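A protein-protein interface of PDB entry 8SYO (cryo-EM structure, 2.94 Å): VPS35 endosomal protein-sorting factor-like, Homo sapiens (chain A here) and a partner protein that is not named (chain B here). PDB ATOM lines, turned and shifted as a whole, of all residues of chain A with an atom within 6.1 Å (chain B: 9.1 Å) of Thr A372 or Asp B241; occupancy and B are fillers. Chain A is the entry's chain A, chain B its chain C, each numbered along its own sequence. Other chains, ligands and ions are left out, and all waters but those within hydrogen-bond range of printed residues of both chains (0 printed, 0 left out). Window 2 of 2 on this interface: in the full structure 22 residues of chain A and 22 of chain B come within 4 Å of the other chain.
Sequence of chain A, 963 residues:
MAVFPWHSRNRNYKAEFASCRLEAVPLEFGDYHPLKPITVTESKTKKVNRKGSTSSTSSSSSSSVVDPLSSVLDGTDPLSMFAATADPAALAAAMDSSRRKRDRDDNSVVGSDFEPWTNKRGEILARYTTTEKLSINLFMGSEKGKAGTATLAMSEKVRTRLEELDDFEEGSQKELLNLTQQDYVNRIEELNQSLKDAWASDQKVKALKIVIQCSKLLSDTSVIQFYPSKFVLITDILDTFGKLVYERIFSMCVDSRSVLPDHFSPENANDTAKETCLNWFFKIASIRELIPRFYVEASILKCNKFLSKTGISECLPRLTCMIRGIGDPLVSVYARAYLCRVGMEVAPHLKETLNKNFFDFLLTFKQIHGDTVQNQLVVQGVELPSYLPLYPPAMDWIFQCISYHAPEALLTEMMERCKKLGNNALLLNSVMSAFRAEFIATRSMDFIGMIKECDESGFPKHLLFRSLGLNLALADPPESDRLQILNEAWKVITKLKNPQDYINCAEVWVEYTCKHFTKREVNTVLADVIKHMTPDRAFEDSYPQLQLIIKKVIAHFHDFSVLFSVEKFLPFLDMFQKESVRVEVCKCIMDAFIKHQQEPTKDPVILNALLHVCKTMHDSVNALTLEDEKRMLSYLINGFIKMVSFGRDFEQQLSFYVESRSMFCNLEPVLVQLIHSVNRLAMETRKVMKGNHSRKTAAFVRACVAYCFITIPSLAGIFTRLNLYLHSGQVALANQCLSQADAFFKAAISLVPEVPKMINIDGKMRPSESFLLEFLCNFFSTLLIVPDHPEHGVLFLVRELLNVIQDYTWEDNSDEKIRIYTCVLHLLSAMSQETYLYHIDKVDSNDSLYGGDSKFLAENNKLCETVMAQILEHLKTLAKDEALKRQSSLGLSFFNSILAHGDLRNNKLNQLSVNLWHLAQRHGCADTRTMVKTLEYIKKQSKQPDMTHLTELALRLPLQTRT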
ATOM      1  N   ILE A 326      25.808 -28.808   8.112  1.00  0.00           N
ATOM      2  CA  ILE A 326      26.364 -28.716   6.766  1.00  0.00           C
ATOM      3  C   ILE A 326      25.207 -28.709   5.771  1.00  0.00           C
ATOM      4  O   ILE A 326      24.511 -29.714   5.607  1.00  0.00           O
ATOM      5  CB  ILE A 326      27.335 -29.864   6.482  1.00  0.00           C
ATOM      6  CG1 ILE A 326      28.427 -29.905   7.550  1.00  0.00           C
ATOM      7  CG2 ILE A 326      27.949 -29.704   5.107  1.00  0.00           C
ATOM      8  CD1 ILE A 326      29.420 -31.017   7.361  1.00  0.00           C
ATOM      9  N   GLY A 327      25.003 -27.574   5.099  1.00  0.00           N
ATOM     10  CA  GLY A 327      23.879 -27.453   4.189  1.00  0.00           C
ATOM     11  C   GLY A 327      24.128 -28.022   2.810  1.00  0.00           C
ATOM     12  O   GLY A 327      23.180 -28.428   2.130  1.00  0.00           O
ATOM     13  N   ASP A 328      25.379 -28.062   2.374  1.00  0.00           N
ATOM     14  CA  ASP A 328      25.688 -28.615   1.063  1.00  0.00           C
ATOM     15  C   ASP A 328      25.601 -30.134   1.127  1.00  0.00           C
ATOM     16  O   ASP A 328      26.289 -30.747   1.949  1.00  0.00           O
ATOM     17  CB  ASP A 328      27.073 -28.185   0.607  1.00  0.00           C
ATOM     18  CG  ASP A 328      27.378 -28.620  -0.812  1.00  0.00           C
ATOM     19  OD1 ASP A 328      26.827 -28.010  -1.751  1.00  0.00           O
ATOM     20  OD2 ASP A 328      28.161 -29.575  -0.991  1.00  0.00           O
ATOM     21  N   GLN A 367      17.672 -32.867  -0.454  1.00  0.00           N
ATOM     22  CA  GLN A 367      18.427 -31.724  -0.950  1.00  0.00           C
ATOM     23  C   GLN A 367      19.243 -32.027  -2.197  1.00  0.00           C
ATOM     24  O   GLN A 367      19.607 -31.091  -2.914  1.00  0.00           O
ATOM     25  CB  GLN A 367      19.366 -31.201   0.136  1.00  0.00           C
ATOM     26  CG  GLN A 367      18.774 -30.121   1.009  1.00  0.00           C
ATOM     27  CD  GLN A 367      19.795 -29.532   1.952  1.00  0.00           C
ATOM     28  OE1 GLN A 367      20.848 -30.121   2.188  1.00  0.00           O
ATOM     29  NE2 GLN A 367      19.491 -28.361   2.500  1.00  0.00           N
ATOM     30  N   GLY A 370      17.273 -30.988  -5.001  1.00  0.00           N
ATOM     31  CA  GLY A 370      16.544 -29.771  -4.706  1.00  0.00           C
ATOM     32  C   GLY A 370      16.921 -28.602  -5.589  1.00  0.00           C
ATOM     33  O   GLY A 370      17.781 -28.724  -6.465  1.00  0.00           O
ATOM     34  N   ASP A 371      16.274 -27.457  -5.362  1.00  0.00           N
ATOM     35  CA  ASP A 371      16.488 -26.296  -6.220  1.00  0.00           C
ATOM     36  C   ASP A 371      17.869 -25.685  -6.011  1.00  0.00           C
ATOM     37  O   ASP A 371      18.526 -25.285  -6.979  1.00  0.00           O
ATOM     38  CB  ASP A 371      15.401 -25.255  -5.967  1.00  0.00           C
ATOM     39  CG  ASP A 371      14.038 -25.710  -6.449  1.00  0.00           C
ATOM     40  OD1 ASP A 371      13.980 -26.498  -7.415  1.00  0.00           O
ATOM     41  OD2 ASP A 371      13.024 -25.279  -5.859  1.00  0.00           O
ATOM     42  N   THR A 372      18.322 -25.602  -4.758  1.00  0.00           N
ATOM     43  CA  THR A 372      19.574 -24.910  -4.460  1.00  0.00           C
ATOM     44  C   THR A 372      20.757 -25.587  -5.142  1.00  0.00           C
ATOM     45  O   THR A 372      21.614 -24.919  -5.736  1.00  0.00           O
ATOM     46  CB  THR A 372      19.789 -24.849  -2.949  1.00  0.00           C
ATOM     47  OG1 THR A 372      18.659 -24.224  -2.329  1.00  0.00           O
ATOM     48  CG2 THR A 372      21.041 -24.055  -2.623  1.00  0.00           C
ATOM     49  N   VAL A 373      20.819 -26.916  -5.071  1.00  0.00           N
ATOM     50  CA  VAL A 373      21.921 -27.636  -5.697  1.00  0.00           C
ATOM     51  C   VAL A 373      21.848 -27.517  -7.213  1.00  0.00           C
ATOM     52  O   VAL A 373      22.878 -27.433  -7.892  1.00  0.00           O
ATOM     53  CB  VAL A 373      21.927 -29.101  -5.235  1.00  0.00           C
ATOM     54  CG1 VAL A 373      23.121 -29.823  -5.810  1.00  0.00           C
ATOM     55  CG2 VAL A 373      21.955 -29.158  -3.729  1.00  0.00           C
ATOM     56  N   GLN A 374      20.636 -27.513  -7.770  1.00  0.00           N
ATOM     57  CA  GLN A 374      20.494 -27.325  -9.210  1.00  0.00           C
ATOM     58  C   GLN A 374      21.017 -25.961  -9.643  1.00  0.00           C
ATOM     59  O   GLN A 374      21.725 -25.850 -10.652  1.00  0.00           O
ATOM     60  CB  GLN A 374      19.032 -27.496  -9.620  1.00  0.00           C
ATOM     61  CG  GLN A 374      18.795 -27.420 -11.117  1.00  0.00           C
ATOM     62  CD  GLN A 374      17.366 -27.747 -11.497  1.00  0.00           C
ATOM     63  OE1 GLN A 374      16.562 -28.145 -10.654  1.00  0.00           O
ATOM     64  NE2 GLN A 374      17.040 -27.583 -12.774  1.00  0.00           N
ATOM     65  N   ASN A 375      20.689 -24.910  -8.888  1.00  0.00           N
ATOM     66  CA  ASN A 375      21.214 -23.585  -9.208  1.00  0.00           C
ATOM     67  C   ASN A 375      22.730 -23.540  -9.065  1.00  0.00           C
ATOM     68  O   ASN A 375      23.417 -22.907  -9.874  1.00  0.00           O
ATOM     69  CB  ASN A 375      20.561 -22.520  -8.328  1.00  0.00           C
ATOM     70  CG  ASN A 375      19.070 -22.396  -8.568  1.00  0.00           C
ATOM     71  OD1 ASN A 375      18.260 -22.685  -7.689  1.00  0.00           O
ATOM     72  ND2 ASN A 375      18.700 -21.966  -9.769  1.00  0.00           N
ATOM     73  N   GLN A 376      23.269 -24.197  -8.038  1.00  0.00           N
ATOM     74  CA  GLN A 376      24.718 -24.235  -7.866  1.00  0.00           C
ATOM     75  C   GLN A 376      25.393 -24.910  -9.055  1.00  0.00           C
ATOM     76  O   GLN A 376      26.407 -24.424  -9.571  1.00  0.00           O
ATOM     77  CB  GLN A 376      25.068 -24.955  -6.563  1.00  0.00           C
ATOM     78  CG  GLN A 376      26.551 -24.987  -6.242  1.00  0.00           C
ATOM     79  CD  GLN A 376      26.865 -25.860  -5.044  1.00  0.00           C
ATOM     80  OE1 GLN A 376      26.710 -27.080  -5.094  1.00  0.00           O
ATOM     81  NE2 GLN A 376      27.309 -25.238  -3.958  1.00  0.00           N
ATOM     82  N   LEU A 377      24.834 -26.033  -9.508  1.00  0.00           N
ATOM     83  CA  LEU A 377      25.382 -26.721 -10.672  1.00  0.00           C
ATOM     84  C   LEU A 377      25.282 -25.860 -11.923  1.00  0.00           C
ATOM     85  O   LEU A 377      26.201 -25.842 -12.749  1.00  0.00           O
ATOM     86  CB  LEU A 377      24.661 -28.049 -10.884  1.00  0.00           C
ATOM     87  CG  LEU A 377      24.923 -29.123  -9.834  1.00  0.00           C
ATOM     88  CD1 LEU A 377      24.002 -30.304 -10.067  1.00  0.00           C
ATOM     89  CD2 LEU A 377      26.375 -29.550  -9.869  1.00  0.00           C
ATOM     90  N   VAL B 199      15.130 -24.251  11.258  1.00  0.00           N
ATOM     91  CA  VAL B 199      14.796 -23.258  10.246  1.00  0.00           C
ATOM     92  C   VAL B 199      13.459 -23.651   9.643  1.00  0.00           C
ATOM     93  O   VAL B 199      13.401 -24.443   8.695  1.00  0.00           O
ATOM     94  CB  VAL B 199      15.888 -23.157   9.167  1.00  0.00           C
ATOM     95  CG1 VAL B 199      15.510 -22.119   8.133  1.00  0.00           C
ATOM     96  CG2 VAL B 199      17.224 -22.824   9.798  1.00  0.00           C
ATOM     97  N   SER B 201      11.154 -21.881   7.935  1.00  0.00           N
ATOM     98  CA  SER B 201      11.010 -21.477   6.538  1.00  0.00           C
ATOM     99  C   SER B 201      11.758 -20.190   6.230  1.00  0.00           C
ATOM    100  O   SER B 201      11.508 -19.164   6.862  1.00  0.00           O
ATOM    101  CB  SER B 201       9.532 -21.304   6.182  1.00  0.00           C
ATOM    102  OG  SER B 201       8.959 -20.224   6.896  1.00  0.00           O
ATOM    103  N   SER B 202      12.651 -20.216   5.246  1.00  0.00           N
ATOM    104  CA  SER B 202      13.387 -19.027   4.841  1.00  0.00           C
ATOM    105  C   SER B 202      13.247 -18.836   3.340  1.00  0.00           C
ATOM    106  O   SER B 202      13.563 -19.743   2.564  1.00  0.00           O
ATOM    107  CB  SER B 202      14.865 -19.127   5.226  1.00  0.00           C
ATOM    108  OG  SER B 202      15.510 -20.160   4.503  1.00  0.00           O
ATOM    109  N   GLU B 203      12.768 -17.658   2.935  1.00  0.00           N
ATOM    110  CA  GLU B 203      12.651 -17.360   1.512  1.00  0.00           C
ATOM    111  C   GLU B 203      14.022 -17.286   0.851  1.00  0.00           C
ATOM    112  O   GLU B 203      14.207 -17.784  -0.266  1.00  0.00           O
ATOM    113  CB  GLU B 203      11.886 -16.055   1.307  1.00  0.00           C
ATOM    114  CG  GLU B 203      11.646 -15.703  -0.151  1.00  0.00           C
ATOM    115  CD  GLU B 203      10.842 -14.430  -0.320  1.00  0.00           C
ATOM    116  OE1 GLU B 203      10.489 -13.809   0.705  1.00  0.00           O
ATOM    117  OE2 GLU B 203      10.563 -14.050  -1.476  1.00  0.00           O
ATOM    118  N   ALA B 204      14.989 -16.674   1.522  1.00  0.00           N
ATOM    119  CA  ALA B 204      16.351 -16.571   1.023  1.00  0.00           C
ATOM    120  C   ALA B 204      17.211 -17.676   1.621  1.00  0.00           C
ATOM    121  O   ALA B 204      16.978 -18.132   2.743  1.00  0.00           O
ATOM    122  CB  ALA B 204      16.953 -15.205   1.350  1.00  0.00           C
ATOM    123  N   ALA B 205      18.205 -18.110   0.852  1.00  0.00           N
ATOM    124  CA  ALA B 205      19.101 -19.157   1.320  1.00  0.00           C
ATOM    125  C   ALA B 205      19.903 -18.673   2.519  1.00  0.00           C
ATOM    126  O   ALA B 205      20.398 -17.543   2.542  1.00  0.00           O
ATOM    127  CB  ALA B 205      20.041 -19.592   0.197  1.00  0.00           C
ATOM    128  N   ILE B 206      20.029 -19.537   3.520  1.00  0.00           N
ATOM    129  CA  ILE B 206      20.750 -19.208   4.743  1.00  0.00           C
ATOM    130  C   ILE B 206      22.226 -19.503   4.513  1.00  0.00           C
ATOM    131  O   ILE B 206      22.614 -20.656   4.308  1.00  0.00           O
ATOM    132  CB  ILE B 206      20.203 -19.987   5.944  1.00  0.00           C
ATOM    133  CG1 ILE B 206      18.868 -19.393   6.388  1.00  0.00           C
ATOM    134  CG2 ILE B 206      21.196 -19.966   7.084  1.00  0.00           C
ATOM    135  CD1 ILE B 206      18.339 -19.981   7.665  1.00  0.00           C
ATOM    136  N   ARG B 207      23.050 -18.457   4.528  1.00  0.00           N
ATOM    137  CA  ARG B 207      24.477 -18.642   4.302  1.00  0.00           C
ATOM    138  C   ARG B 207      25.162 -19.238   5.525  1.00  0.00           C
ATOM    139  O   ARG B 207      25.997 -20.139   5.395  1.00  0.00           O
ATOM    140  CB  ARG B 207      25.123 -17.311   3.922  1.00  0.00           C
ATOM    141  CG  ARG B 207      26.574 -17.431   3.499  1.00  0.00           C
ATOM    142  CD  ARG B 207      27.190 -16.065   3.263  1.00  0.00           C
ATOM    143  NE  ARG B 207      26.629 -15.407   2.091  1.00  0.00           N
ATOM    144  CZ  ARG B 207      26.872 -14.148   1.753  1.00  0.00           C
ATOM    145  NH1 ARG B 207      27.663 -13.379   2.482  1.00  0.00           N
ATOM    146  NH2 ARG B 207      26.307 -13.650   0.658  1.00  0.00           N
ATOM    147  N   SER B 208      24.821 -18.757   6.719  1.00  0.00           N
ATOM    148  CA  SER B 208      25.498 -19.209   7.926  1.00  0.00           C
ATOM    149  C   SER B 208      24.691 -18.810   9.151  1.00  0.00           C
ATOM    150  O   SER B 208      24.138 -17.711   9.205  1.00  0.00           O
ATOM    151  CB  SER B 208      26.910 -18.622   8.020  1.00  0.00           C
ATOM    152  OG  SER B 208      27.556 -19.037   9.209  1.00  0.00           O
ATOM    153  N   VAL B 209      24.632 -19.715  10.125  1.00  0.00           N
ATOM    154  CA  VAL B 209      24.088 -19.444  11.449  1.00  0.00           C
ATOM    155  C   VAL B 209      25.177 -19.769  12.460  1.00  0.00           C
ATOM    156  O   VAL B 209      25.673 -20.902  12.493  1.00  0.00           O
ATOM    157  CB  VAL B 209      22.823 -20.264  11.745  1.00  0.00           C
ATOM    158  CG1 VAL B 209      22.179 -19.779  13.027  1.00  0.00           C
ATOM    159  CG2 VAL B 209      21.850 -20.176  10.593  1.00  0.00           C
ATOM    160  N   GLN B 236      30.344 -21.226  14.486  1.00  0.00           N
ATOM    161  CA  GLN B 236      29.340 -21.486  13.469  1.00  0.00           C
ATOM    162  C   GLN B 236      28.713 -22.855  13.683  1.00  0.00           C
ATOM    163  O   GLN B 236      29.409 -23.846  13.918  1.00  0.00           O
ATOM    164  CB  GLN B 236      29.971 -21.410  12.081  1.00  0.00           C
ATOM    165  CG  GLN B 236      28.988 -21.404  10.935  1.00  0.00           C
ATOM    166  CD  GLN B 236      29.672 -21.601   9.601  1.00  0.00           C
ATOM    167  OE1 GLN B 236      30.787 -22.111   9.538  1.00  0.00           O
ATOM    168  NE2 GLN B 236      29.014 -21.188   8.529  1.00  0.00           N
ATOM    169  N   ALA B 238      25.601 -23.700  11.593  1.00  0.00           N
ATOM    170  CA  ALA B 238      24.932 -24.069  10.351  1.00  0.00           C
ATOM    171  C   ALA B 238      25.655 -23.406   9.191  1.00  0.00           C
ATOM    172  O   ALA B 238      25.775 -22.180   9.158  1.00  0.00           O
ATOM    173  CB  ALA B 238      23.459 -23.659  10.373  1.00  0.00           C
ATOM    174  N   ASP B 239      26.126 -24.213   8.244  1.00  0.00           N
ATOM    175  CA  ASP B 239      26.836 -23.730   7.069  1.00  0.00           C
ATOM    176  C   ASP B 239      26.057 -24.116   5.823  1.00  0.00           C
ATOM    177  O   ASP B 239      25.719 -25.290   5.637  1.00  0.00           O
ATOM    178  CB  ASP B 239      28.251 -24.307   7.006  1.00  0.00           C
ATOM    179  CG  ASP B 239      29.079 -23.703   5.891  1.00  0.00           C
ATOM    180  OD1 ASP B 239      28.697 -22.630   5.377  1.00  0.00           O
ATOM    181  OD2 ASP B 239      30.114 -24.300   5.528  1.00  0.00           O
ATOM    182  N   GLY B 240      25.774 -23.134   4.973  1.00  0.00           N
ATOM    183  CA  GLY B 240      25.004 -23.381   3.774  1.00  0.00           C
ATOM    184  C   GLY B 240      23.518 -23.473   4.054  1.00  0.00           C
ATOM    185  O   GLY B 240      23.045 -23.330   5.182  1.00  0.00           O
ATOM    186  N   ASP B 241      22.764 -23.721   2.987  1.00  0.00           N
ATOM    187  CA  ASP B 241      21.308 -23.799   3.071  1.00  0.00           C
ATOM    188  C   ASP B 241      20.919 -25.099   3.761  1.00  0.00           C
ATOM    189  O   ASP B 241      20.959 -26.175   3.161  1.00  0.00           O
ATOM    190  CB  ASP B 241      20.690 -23.705   1.683  1.00  0.00           C
ATOM    191  CG  ASP B 241      19.262 -23.207   1.717  1.00  0.00           C
ATOM    192  OD1 ASP B 241      18.794 -22.827   2.810  1.00  0.00           O
ATOM    193  OD2 ASP B 241      18.607 -23.196   0.653  1.00  0.00           O
ATOM    194  N   VAL B 242      20.540 -25.001   5.029  1.00  0.00           N
ATOM    195  CA  VAL B 242      20.178 -26.170   5.819  1.00  0.00           C
ATOM    196  C   VAL B 242      18.753 -26.587   5.480  1.00  0.00           C
ATOM    197  O   VAL B 242      17.919 -25.762   5.091  1.00  0.00           O
ATOM    198  CB  VAL B 242      20.348 -25.856   7.320  1.00  0.00           C
ATOM    199  CG1 VAL B 242      19.970 -27.050   8.178  1.00  0.00           C
ATOM    200  CG2 VAL B 242      21.769 -25.419   7.604  1.00  0.00           C
ATOM    201  N   CYS B 243      18.472 -27.884   5.612  1.00  0.00           N
ATOM    202  CA  CYS B 243      17.142 -28.401   5.319  1.00  0.00           C
ATOM    203  C   CYS B 243      16.092 -27.710   6.180  1.00  0.00           C
ATOM    204  O   CYS B 243      16.296 -27.478   7.375  1.00  0.00           O
ATOM    205  CB  CYS B 243      17.091 -29.909   5.557  1.00  0.00           C
ATOM    206  SG  CYS B 243      18.291 -30.871   4.619  1.00  0.00           S
ATOM    207  N   ARG B 244      14.961 -27.384   5.562  1.00  0.00           N
ATOM    208  CA  ARG B 244      13.879 -26.682   6.243  1.00  0.00           C
ATOM    209  C   ARG B 244      13.099 -27.681   7.084  1.00  0.00           C
ATOM    210  O   ARG B 244      12.359 -28.512   6.547  1.00  0.00           O
ATOM    211  CB  ARG B 244      12.978 -25.991   5.228  1.00  0.00           C
ATOM    212  CG  ARG B 244      13.733 -25.163   4.209  1.00  0.00           C
ATOM    213  CD  ARG B 244      14.034 -23.779   4.741  1.00  0.00           C
ATOM    214  NE  ARG B 244      14.581 -22.907   3.711  1.00  0.00           N
ATOM    215  CZ  ARG B 244      15.826 -22.966   3.263  1.00  0.00           C
ATOM    216  NH1 ARG B 244      16.691 -23.847   3.738  1.00  0.00           N
ATOM    217  NH2 ARG B 244      16.216 -22.119   2.315  1.00  0.00           N
ATOM    218  N   LEU B 246      14.879 -29.298   9.862  1.00  0.00           N
ATOM    219  CA  LEU B 246      15.873 -30.128  10.525  1.00  0.00           C
ATOM    220  C   LEU B 246      16.443 -29.381  11.720  1.00  0.00           C
ATOM    221  O   LEU B 246      16.779 -28.198  11.623  1.00  0.00           O
ATOM    222  CB  LEU B 246      16.993 -30.510   9.560  1.00  0.00           C
ATOM    223  CG  LEU B 246      17.718 -31.816   9.870  1.00  0.00           C
ATOM    224  CD1 LEU B 246      16.776 -32.990   9.707  1.00  0.00           C
ATOM    225  CD2 LEU B 246      18.926 -31.973   8.967  1.00  0.00           C
ATOM    226  N   VAL B 248      19.070 -28.291  13.739  1.00  0.00           N
ATOM    227  CA  VAL B 248      20.517 -28.094  13.871  1.00  0.00           C
ATOM    228  C   VAL B 248      20.872 -28.021  15.350  1.00  0.00           C
ATOM    229  O   VAL B 248      20.225 -27.269  16.103  1.00  0.00           O
ATOM    230  CB  VAL B 248      20.948 -26.825  13.141  1.00  0.00           C
ATOM    231  CG1 VAL B 248      22.462 -26.713  13.115  1.00  0.00           C
ATOM    232  CG2 VAL B 248      20.383 -26.811  11.739  1.00  0.00           C
ATOM    233  N   LEU B 279      22.786 -15.301   9.010  1.00  0.00           N
ATOM    234  CA  LEU B 279      23.230 -14.621   7.805  1.00  0.00           C
ATOM    235  C   LEU B 279      22.472 -15.183   6.613  1.00  0.00           C
ATOM    236  O   LEU B 279      22.411 -16.402   6.430  1.00  0.00           O
ATOM    237  CB  LEU B 279      24.737 -14.788   7.607  1.00  0.00           C
ATOM    238  CG  LEU B 279      25.477 -13.618   6.960  1.00  0.00           C
ATOM    239  CD1 LEU B 279      25.411 -12.389   7.849  1.00  0.00           C
ATOM    240  CD2 LEU B 279      26.920 -13.993   6.665  1.00  0.00           C
ATOM    241  N   LEU B 280      21.893 -14.298   5.814  1.00  0.00           N
ATOM    242  CA  LEU B 280      21.151 -14.677   4.623  1.00  0.00           C
ATOM    243  C   LEU B 280      21.992 -14.410   3.380  1.00  0.00           C
ATOM    244  O   LEU B 280      23.067 -13.810   3.442  1.00  0.00           O
ATOM    245  CB  LEU B 280      19.819 -13.926   4.555  1.00  0.00           C
ATOM    246  CG  LEU B 280      18.637 -14.503   5.343  1.00  0.00           C
ATOM    247  CD1 LEU B 280      18.265 -15.879   4.819  1.00  0.00           C
ATOM    248  CD2 LEU B 280      18.901 -14.551   6.839  1.00  0.00           C
ATOM    249  N   HIS B 281      21.490 -14.877   2.238  1.00  0.00           N
ATOM    250  CA  HIS B 281      22.283 -14.838   1.010  1.00  0.00           C
ATOM    251  C   HIS B 281      22.667 -13.426   0.578  1.00  0.00           C
ATOM    252  O   HIS B 281      23.855 -13.201   0.286  1.00  0.00           O
ATOM    253  CB  HIS B 281      21.542 -15.577  -0.108  1.00  0.00           C
ATOM    254  CG  HIS B 281      21.897 -15.099  -1.481  1.00  0.00           C
ATOM    255  ND1 HIS B 281      23.136 -15.310  -2.045  1.00  0.00           N
ATOM    256  CD2 HIS B 281      21.175 -14.419  -2.402  1.00  0.00           C
ATOM    257  CE1 HIS B 281      23.163 -14.783  -3.254  1.00  0.00           C
ATOM    258  NE2 HIS B 281      21.986 -14.234  -3.496  1.00  0.00           N
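OG1 of Thr A372 lies within hydrogen-bond range of OD2 of Asp B241 (3.2 Å). The backbone carbonyl oxygen (O) of Gly A327 sits close to the backbone carbonyl oxygen (O) of Asp B241. NE2 of Gln A367 sits at hydrogen-bond distance from O of Asp B241 (2.7 Å). The side-chain amide nitrogen of Gln A367 lies close to the backbone NH of Cys B243 (3.3 Å). The backbone NH of Gly A327 lies within hydrogen-bond range of the backbone carbonyl oxygen of Asp B239, at 2.5 Å.
NH1 of Arg B244 lies within salt-bridge range of OD1 of Asp B241 (2.5 Å). O of Val B242 lies within hydrogen-bond range of NH1 of Arg B244 (2.6 Å). The side-chain amide oxygen (OE1) of Gln A367 sits close to the backbone carbonyl oxygen (O) of Gly A327 (2.9 Å). The backbone NH (N) of Gly B240 is in hydrogen-bond range of the backbone carbonyl oxygen (O) of Arg B207 (3.0 Å). O of Ile B206 is in hydrogen-bond range of N of Asp B241 (3.3 Å). The side-chain amide nitrogen of Gln B236 lies within hydrogen-bond range of the side-chain carboxylate of Asp B239 (3.5 Å).
Among the printed residues, pairs that only touch across the chains: Ile A326 with Asp B239 (3.5 Å), Gly A327 with Gly B240 (3.999 Å) and Gln A367 with Val B242 (3.5 Å).
Asp B241 touches just these residues of chain A: Gly A327 (3.3 Å), Gln A367 (2.7 Å) and Thr A372 (3.2 Å). Of the printed residues of chain A, Gly B240 touches Gly A327 (3.999 Å). Printed residues of chain A within 4 Å of Val B242: Gln A367. Printed residues of chain A within 4 Å of Asp B239: Ile A326 (3.5 Å) and Gly A327 (2.5 Å). Of the printed residues of chain B, Gly A327 touches Asp B239 (2.5 Å), Gly B240 (3.999 Å) and Asp B241 (3.3 Å). Of the printed residues of chain B, Ile A326 touches Asp B239 (3.5 Å). The nearest residue of chain A that does not touch Asp B241 is Asp A328 (4.9 Å). The nearest printed residue of chain B that does not touch Ile A326 is Val B242 (5.1 Å).
Printed residues of chain A that touch a printed residue of chain B: Ile A326, Gly A327, Gln A367 and Thr A372. Among the printed residues, no Asp or Glu carboxylate lies within 4 Å of a Lys or Arg side-chain nitrogen of the other chain.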
